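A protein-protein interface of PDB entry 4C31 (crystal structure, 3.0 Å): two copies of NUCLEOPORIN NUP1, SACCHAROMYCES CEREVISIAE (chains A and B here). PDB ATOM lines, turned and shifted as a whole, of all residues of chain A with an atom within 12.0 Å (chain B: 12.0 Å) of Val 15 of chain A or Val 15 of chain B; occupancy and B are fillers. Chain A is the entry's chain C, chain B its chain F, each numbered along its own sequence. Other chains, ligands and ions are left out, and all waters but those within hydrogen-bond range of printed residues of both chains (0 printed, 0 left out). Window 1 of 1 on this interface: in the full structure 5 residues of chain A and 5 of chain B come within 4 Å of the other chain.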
ATOM      1  N   ILE A  10     -13.933  -7.495  -8.960  1.00  0.00           N
ATOM      2  CA  ILE A  10     -12.780  -6.837  -9.567  1.00  0.00           C
ATOM      3  C   ILE A  10     -11.474  -7.325  -8.943  1.00  0.00           C
ATOM      4  O   ILE A  10     -11.391  -7.585  -7.738  1.00  0.00           O
ATOM      5  CB  ILE A  10     -12.871  -5.293  -9.450  1.00  0.00           C
ATOM      6  CG1 ILE A  10     -13.944  -4.769 -10.409  1.00  0.00           C
ATOM      7  CG2 ILE A  10     -11.527  -4.630  -9.788  1.00  0.00           C
ATOM      8  CD1 ILE A  10     -14.131  -3.256 -10.408  1.00  0.00           C
ATOM      9  N   VAL A  11     -10.461  -7.451  -9.794  1.00  0.00           N
ATOM     10  CA  VAL A  11      -9.139  -7.907  -9.388  1.00  0.00           C
ATOM     11  C   VAL A  11      -8.365  -6.785  -8.702  1.00  0.00           C
ATOM     12  O   VAL A  11      -8.021  -5.789  -9.337  1.00  0.00           O
ATOM     13  CB  VAL A  11      -8.338  -8.417 -10.617  1.00  0.00           C
ATOM     14  CG1 VAL A  11      -6.890  -8.736 -10.252  1.00  0.00           C
ATOM     15  CG2 VAL A  11      -9.023  -9.635 -11.223  1.00  0.00           C
ATOM     16  N   LEU A  12      -8.089  -6.948  -7.411  1.00  0.00           N
ATOM     17  CA  LEU A  12      -7.268  -5.980  -6.691  1.00  0.00           C
ATOM     18  C   LEU A  12      -5.806  -6.407  -6.646  1.00  0.00           C
ATOM     19  O   LEU A  12      -5.510  -7.594  -6.492  1.00  0.00           O
ATOM     20  CB  LEU A  12      -7.785  -5.785  -5.273  1.00  0.00           C
ATOM     21  CG  LEU A  12      -8.808  -4.661  -5.150  1.00  0.00           C
ATOM     22  CD1 LEU A  12     -10.121  -5.043  -5.825  1.00  0.00           C
ATOM     23  CD2 LEU A  12      -9.017  -4.328  -3.692  1.00  0.00           C
ATOM     24  N   PRO A  13      -4.881  -5.439  -6.769  1.00  0.00           N
ATOM     25  CA  PRO A  13      -3.466  -5.795  -6.610  1.00  0.00           C
ATOM     26  C   PRO A  13      -3.135  -6.258  -5.196  1.00  0.00           C
ATOM     27  O   PRO A  13      -3.812  -5.862  -4.247  1.00  0.00           O
ATOM     28  CB  PRO A  13      -2.723  -4.489  -6.941  1.00  0.00           C
ATOM     29  CG  PRO A  13      -3.744  -3.410  -6.915  1.00  0.00           C
ATOM     30  CD  PRO A  13      -5.063  -4.043  -7.205  1.00  0.00           C
ATOM     31  N   THR A  14      -2.108  -7.095  -5.066  1.00  0.00           N
ATOM     32  CA  THR A  14      -1.667  -7.567  -3.765  1.00  0.00           C
ATOM     33  C   THR A  14      -0.829  -6.501  -3.078  1.00  0.00           C
ATOM     34  O   THR A  14      -0.490  -5.483  -3.678  1.00  0.00           O
ATOM     35  CB  THR A  14      -0.823  -8.850  -3.860  1.00  0.00           C
ATOM     36  OG1 THR A  14       0.495  -8.532  -4.321  1.00  0.00           O
ATOM     37  CG2 THR A  14      -1.468  -9.855  -4.789  1.00  0.00           C
ATOM     38  N   VAL A  15      -0.473  -6.764  -1.825  1.00  0.00           N
ATOM     39  CA  VAL A  15       0.354  -5.851  -1.048  1.00  0.00           C
ATOM     40  C   VAL A  15       1.697  -5.614  -1.752  1.00  0.00           C
ATOM     41  O   VAL A  15       2.357  -4.596  -1.531  1.00  0.00           O
ATOM     42  CB  VAL A  15       0.582  -6.402   0.381  1.00  0.00           C
ATOM     43  CG1 VAL A  15       1.361  -7.712   0.341  1.00  0.00           C
ATOM     44  CG2 VAL A  15       1.287  -5.371   1.258  1.00  0.00           C
ATOM     45  N   GLY A  16       2.083  -6.555  -2.613  1.00  0.00           N
ATOM     46  CA  GLY A  16       3.343  -6.483  -3.337  1.00  0.00           C
ATOM     47  C   GLY A  16       3.387  -5.378  -4.380  1.00  0.00           C
ATOM     48  O   GLY A  16       4.464  -4.968  -4.814  1.00  0.00           O
ATOM     49  N   PHE A  17       2.213  -4.923  -4.809  1.00  0.00           N
ATOM     50  CA  PHE A  17       2.111  -3.844  -5.782  1.00  0.00           C
ATOM     51  C   PHE A  17       2.295  -2.478  -5.113  1.00  0.00           C
ATOM     52  O   PHE A  17       1.323  -1.834  -4.716  1.00  0.00           O
ATOM     53  CB  PHE A  17       0.761  -3.913  -6.493  1.00  0.00           C
ATOM     54  CG  PHE A  17       0.627  -2.945  -7.629  1.00  0.00           C
ATOM     55  CD1 PHE A  17       1.171  -3.236  -8.870  1.00  0.00           C
ATOM     56  CD2 PHE A  17      -0.047  -1.747  -7.459  1.00  0.00           C
ATOM     57  CE1 PHE A  17       1.048  -2.350  -9.916  1.00  0.00           C
ATOM     58  CE2 PHE A  17      -0.172  -0.857  -8.498  1.00  0.00           C
ATOM     59  CZ  PHE A  17       0.375  -1.157  -9.731  1.00  0.00           C
ATOM     60  N   ASP A  18       3.545  -2.037  -4.999  1.00  0.00           N
ATOM     61  CA  ASP A  18       3.871  -0.851  -4.213  1.00  0.00           C
ATOM     62  C   ASP A  18       4.016   0.410  -5.059  1.00  0.00           C
ATOM     63  O   ASP A  18       5.056   1.072  -5.030  1.00  0.00           O
ATOM     64  CB  ASP A  18       5.165  -1.090  -3.430  1.00  0.00           C
ATOM     65  CG  ASP A  18       6.343  -1.403  -4.330  1.00  0.00           C
ATOM     66  OD1 ASP A  18       6.113  -1.792  -5.494  1.00  0.00           O
ATOM     67  OD2 ASP A  18       7.498  -1.263  -3.873  1.00  0.00           O
ATOM     68  N   PHE A  19       2.972   0.753  -5.802  1.00  0.00           N
ATOM     69  CA  PHE A  19       2.990   1.977  -6.590  1.00  0.00           C
ATOM     70  C   PHE A  19       3.081   3.187  -5.667  1.00  0.00           C
ATOM     71  O   PHE A  19       3.918   4.066  -5.862  1.00  0.00           O
ATOM     72  CB  PHE A  19       1.744   2.079  -7.470  1.00  0.00           C
ATOM     73  CG  PHE A  19       1.705   3.314  -8.328  1.00  0.00           C
ATOM     74  CD1 PHE A  19       2.851   3.785  -8.950  1.00  0.00           C
ATOM     75  CD2 PHE A  19       0.519   4.011  -8.510  1.00  0.00           C
ATOM     76  CE1 PHE A  19       2.814   4.919  -9.742  1.00  0.00           C
ATOM     77  CE2 PHE A  19       0.476   5.148  -9.297  1.00  0.00           C
ATOM     78  CZ  PHE A  19       1.625   5.603  -9.914  1.00  0.00           C
ATOM     79  N   ILE A  20       2.210   3.212  -4.660  1.00  0.00           N
ATOM     80  CA  ILE A  20       2.180   4.291  -3.677  1.00  0.00           C
ATOM     81  C   ILE A  20       2.993   3.929  -2.431  1.00  0.00           C
ATOM     82  O   ILE A  20       2.723   2.920  -1.774  1.00  0.00           O
ATOM     83  CB  ILE A  20       0.735   4.630  -3.251  1.00  0.00           C
ATOM     84  CG1 ILE A  20      -0.210   4.574  -4.459  1.00  0.00           C
ATOM     85  CG2 ILE A  20       0.699   6.002  -2.584  1.00  0.00           C
ATOM     86  CD1 ILE A  20      -1.665   4.833  -4.122  1.00  0.00           C
ATOM     87  N   LYS A  21       3.991   4.757  -2.127  1.00  0.00           N
ATOM     88  CA  LYS A  21       4.901   4.526  -1.002  1.00  0.00           C
ATOM     89  C   LYS A  21       5.650   3.212  -1.174  1.00  0.00           C
ATOM     90  O   LYS A  21       6.464   3.071  -2.087  1.00  0.00           O
ATOM     91  CB  LYS A  21       4.142   4.536   0.331  1.00  0.00           C
ATOM     92  CG  LYS A  21       3.320   5.795   0.559  1.00  0.00           C
ATOM     93  CD  LYS A  21       2.525   5.727   1.851  1.00  0.00           C
ATOM     94  CE  LYS A  21       1.726   7.001   2.072  1.00  0.00           C
ATOM     95  NZ  LYS A  21       2.589   8.216   2.075  1.00  0.00           N
ATOM     96  N   ILE B  10      -1.492 -19.944  -0.407  1.00  0.00           N
ATOM     97  CA  ILE B  10      -1.549 -19.024   0.722  1.00  0.00           C
ATOM     98  C   ILE B  10      -2.218 -17.711   0.321  1.00  0.00           C
ATOM     99  O   ILE B  10      -2.036 -17.199  -0.793  1.00  0.00           O
ATOM    100  CB  ILE B  10      -0.139 -18.754   1.304  1.00  0.00           C
ATOM    101  CG1 ILE B  10       0.383 -20.015   1.999  1.00  0.00           C
ATOM    102  CG2 ILE B  10      -0.168 -17.585   2.298  1.00  0.00           C
ATOM    103  CD1 ILE B  10       1.768 -19.880   2.613  1.00  0.00           C
ATOM    104  N   VAL B  11      -2.995 -17.190   1.264  1.00  0.00           N
ATOM    105  CA  VAL B  11      -3.753 -15.958   1.104  1.00  0.00           C
ATOM    106  C   VAL B  11      -2.849 -14.741   1.249  1.00  0.00           C
ATOM    107  O   VAL B  11      -2.319 -14.498   2.329  1.00  0.00           O
ATOM    108  CB  VAL B  11      -4.888 -15.886   2.164  1.00  0.00           C
ATOM    109  CG1 VAL B  11      -5.607 -14.534   2.131  1.00  0.00           C
ATOM    110  CG2 VAL B  11      -5.877 -17.031   1.963  1.00  0.00           C
ATOM    111  N   LEU B  12      -2.680 -13.970   0.180  1.00  0.00           N
ATOM    112  CA  LEU B  12      -1.890 -12.741   0.272  1.00  0.00           C
ATOM    113  C   LEU B  12      -2.776 -11.528   0.552  1.00  0.00           C
ATOM    114  O   LEU B  12      -3.899 -11.452   0.061  1.00  0.00           O
ATOM    115  CB  LEU B  12      -1.087 -12.514  -1.006  1.00  0.00           C
ATOM    116  CG  LEU B  12       0.308 -13.136  -0.963  1.00  0.00           C
ATOM    117  CD1 LEU B  12       0.242 -14.664  -1.005  1.00  0.00           C
ATOM    118  CD2 LEU B  12       1.130 -12.596  -2.104  1.00  0.00           C
ATOM    119  N   PRO B  13      -2.287 -10.589   1.376  1.00  0.00           N
ATOM    120  CA  PRO B  13      -3.058  -9.356   1.579  1.00  0.00           C
ATOM    121  C   PRO B  13      -3.130  -8.495   0.324  1.00  0.00           C
ATOM    122  O   PRO B  13      -2.241  -8.562  -0.529  1.00  0.00           O
ATOM    123  CB  PRO B  13      -2.295  -8.626   2.691  1.00  0.00           C
ATOM    124  CG  PRO B  13      -0.959  -9.279   2.767  1.00  0.00           C
ATOM    125  CD  PRO B  13      -1.111 -10.670   2.261  1.00  0.00           C
ATOM    126  N   THR B  14      -4.182  -7.692   0.217  1.00  0.00           N
ATOM    127  CA  THR B  14      -4.324  -6.783  -0.911  1.00  0.00           C
ATOM    128  C   THR B  14      -3.442  -5.557  -0.725  1.00  0.00           C
ATOM    129  O   THR B  14      -2.797  -5.381   0.308  1.00  0.00           O
ATOM    130  CB  THR B  14      -5.777  -6.319  -1.104  1.00  0.00           C
ATOM    131  OG1 THR B  14      -6.117  -5.369  -0.087  1.00  0.00           O
ATOM    132  CG2 THR B  14      -6.735  -7.499  -1.048  1.00  0.00           C
ATOM    133  N   VAL B  15      -3.412  -4.715  -1.751  1.00  0.00           N
ATOM    134  CA  VAL B  15      -2.642  -3.482  -1.718  1.00  0.00           C
ATOM    135  C   VAL B  15      -3.119  -2.580  -0.569  1.00  0.00           C
ATOM    136  O   VAL B  15      -2.367  -1.737  -0.077  1.00  0.00           O
ATOM    137  CB  VAL B  15      -2.746  -2.744  -3.081  1.00  0.00           C
ATOM    138  CG1 VAL B  15      -4.187  -2.318  -3.362  1.00  0.00           C
ATOM    139  CG2 VAL B  15      -1.791  -1.552  -3.141  1.00  0.00           C
ATOM    140  N   GLY B  16      -4.361  -2.777  -0.133  1.00  0.00           N
ATOM    141  CA  GLY B  16      -4.936  -1.969   0.929  1.00  0.00           C
ATOM    142  C   GLY B  16      -4.332  -2.216   2.303  1.00  0.00           C
ATOM    143  O   GLY B  16      -4.391  -1.347   3.172  1.00  0.00           O
ATOM    144  N   PHE B  17      -3.732  -3.386   2.496  1.00  0.00           N
ATOM    145  CA  PHE B  17      -3.126  -3.735   3.777  1.00  0.00           C
ATOM    146  C   PHE B  17      -1.768  -3.064   3.912  1.00  0.00           C
ATOM    147  O   PHE B  17      -0.740  -3.657   3.588  1.00  0.00           O
ATOM    148  CB  PHE B  17      -2.992  -5.255   3.895  1.00  0.00           C
ATOM    149  CG  PHE B  17      -2.549  -5.726   5.248  1.00  0.00           C
ATOM    150  CD1 PHE B  17      -3.458  -5.846   6.281  1.00  0.00           C
ATOM    151  CD2 PHE B  17      -1.227  -6.063   5.480  1.00  0.00           C
ATOM    152  CE1 PHE B  17      -3.057  -6.285   7.527  1.00  0.00           C
ATOM    153  CE2 PHE B  17      -0.820  -6.501   6.721  1.00  0.00           C
ATOM    154  CZ  PHE B  17      -1.735  -6.613   7.749  1.00  0.00           C
ATOM    155  N   ASP B  18      -1.767  -1.834   4.416  1.00  0.00           N
ATOM    156  CA  ASP B  18      -0.569  -0.997   4.391  1.00  0.00           C
ATOM    157  C   ASP B  18       0.226  -1.044   5.689  1.00  0.00           C
ATOM    158  O   ASP B  18       0.470  -0.016   6.318  1.00  0.00           O
ATOM    159  CB  ASP B  18      -0.950   0.450   4.070  1.00  0.00           C
ATOM    160  CG  ASP B  18      -1.922   1.036   5.072  1.00  0.00           C
ATOM    161  OD1 ASP B  18      -2.587   0.257   5.784  1.00  0.00           O
ATOM    162  OD2 ASP B  18      -2.019   2.278   5.151  1.00  0.00           O
ATOM    163  N   PHE B  19       0.669  -2.236   6.068  1.00  0.00           N
ATOM    164  CA  PHE B  19       1.471  -2.390   7.270  1.00  0.00           C
ATOM    165  C   PHE B  19       2.773  -1.597   7.141  1.00  0.00           C
ATOM    166  O   PHE B  19       3.100  -0.803   8.019  1.00  0.00           O
ATOM    167  CB  PHE B  19       1.744  -3.876   7.533  1.00  0.00           C
ATOM    168  CG  PHE B  19       2.557  -4.139   8.771  1.00  0.00           C
ATOM    169  CD1 PHE B  19       2.361  -3.388   9.919  1.00  0.00           C
ATOM    170  CD2 PHE B  19       3.499  -5.157   8.793  1.00  0.00           C
ATOM    171  CE1 PHE B  19       3.106  -3.628  11.057  1.00  0.00           C
ATOM    172  CE2 PHE B  19       4.243  -5.406   9.929  1.00  0.00           C
ATOM    173  CZ  PHE B  19       4.046  -4.641  11.063  1.00  0.00           C
ATOM    174  N   ILE B  20       3.489  -1.771   6.033  1.00  0.00           N
ATOM    175  CA  ILE B  20       4.717  -1.009   5.801  1.00  0.00           C
ATOM    176  C   ILE B  20       4.391   0.242   4.990  1.00  0.00           C
ATOM    177  O   ILE B  20       3.891   0.151   3.868  1.00  0.00           O
ATOM    178  CB  ILE B  20       5.793  -1.828   5.061  1.00  0.00           C
ATOM    179  CG1 ILE B  20       5.868  -3.254   5.609  1.00  0.00           C
ATOM    180  CG2 ILE B  20       7.150  -1.155   5.203  1.00  0.00           C
ATOM    181  CD1 ILE B  20       5.198  -4.270   4.729  1.00  0.00           C
ATOM    182  N   LYS B  21       4.695   1.402   5.574  1.00  0.00           N
ATOM    183  CA  LYS B  21       4.362   2.702   4.993  1.00  0.00           C
ATOM    184  C   LYS B  21       2.850   2.849   4.847  1.00  0.00           C
ATOM    185  O   LYS B  21       2.135   3.002   5.839  1.00  0.00           O
ATOM    186  CB  LYS B  21       5.051   2.896   3.639  1.00  0.00           C
ATOM    187  CG  LYS B  21       6.556   2.713   3.690  1.00  0.00           C
ATOM    188  CD  LYS B  21       7.188   2.839   2.313  1.00  0.00           C
ATOM    189  CE  LYS B  21       8.699   2.700   2.384  1.00  0.00           C
ATOM    190  NZ  LYS B  21       9.104   1.437   3.059  1.00  0.00           N
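Of the 12 printed residues of chain B, 5 touch a printed residue of chain A.
Among the printed residues, 11 pairs touch across the chains.
N of Gly 16 of chain A lies close to OG1 of Thr 14 of chain A (3.1 Å).
The backbone NH (N) of Gly 16 of chain B lies close to the side-chain hydroxyl (OG1) of Thr 14 of chain B (3.1 Å).
Pro 13 of chain A touches Val 15 of chain B, and with the chains exchanged Val 15 of chain A touches Pro 13 of chain B.
Thr 14 of chain B touches its own counterpart, Thr 14 of chain A.
Val 15 of chain B touches its own counterpart, Val 15 of chain A.
Lys 21 of chain B touches its own counterpart, Lys 21 of chain A.
Positions printed for both chains: 10, 11, 12, 13, 14, 15, 16, 17, 18, 19, 20 and 21.
Of the 11 pairs that touch across the chains among the printed residues, 11 have their exchanged pair printed and touching as well.
Of chain B, only Pro 13, Thr 14, Val 15 and Phe 17 come within 4 Å of Val 15 of chain A.
Of chain A, only Pro 13, Thr 14, Val 15 and Phe 17 come within 4 Å of Val 15 of chain B.
No residue of chain B comes within 4 Å of Leu 12 of chain A.
Thr 14 of chain A touches just these residues of chain B: Pro 13, Thr 14 and Val 15.
Phe 17 of chain A touches just one residue of chain B: Val 15.
Of chain A, only Pro 13 (3.5 Å), Thr 14 (3.6 Å) and Val 15 (3.4 Å) come within 4 Å of Thr 14 of chain B.
No residue of chain A comes within 4 Å of Gly 16 of chain B.
No residue of chain A comes within 4 Å of Asp 18 of chain B.
Printed residues of chain B within 4 Å of Lys 21 of chain A: Lys 21.
Of the printed residues of chain A, Lys 21 of chain B touches Lys 21.
The nearest residue of chain B that does not touch Val 15 of chain A is Ile 20 of chain B (5.3 Å).
The nearest residue of chain A that does not touch Val 15 of chain B is Leu 12 of chain A (5.2 Å).
N of Val 15 of chain B lies within hydrogen-bond range of O of Pro 13 of chain A (2.8 Å).
The backbone carbonyl oxygen (O) of Pro 13 of chain B lies within hydrogen-bond range of the backbone NH (N) of Val 15 of chain A, 2.8 Å away.
N of Val 15 of chain A sits close to O of Thr 14 of chain B.
Among the printed residues, merely in contact across the chains: Pro 13 of chain A with Thr 14 of chain B, Thr 14 of chain A with Pro 13 of chain B, Thr 14 of chain A with Thr 14 of chain B, Thr 14 of chain A with Val 15 of chain B, Val 15 of chain A with Val 15 of chain B, Val 15 of chain A with Phe 17 of chain B, Phe 17 of chain A with Val 15 of chain B and Lys 21 of chain A with Lys 21 of chain B.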
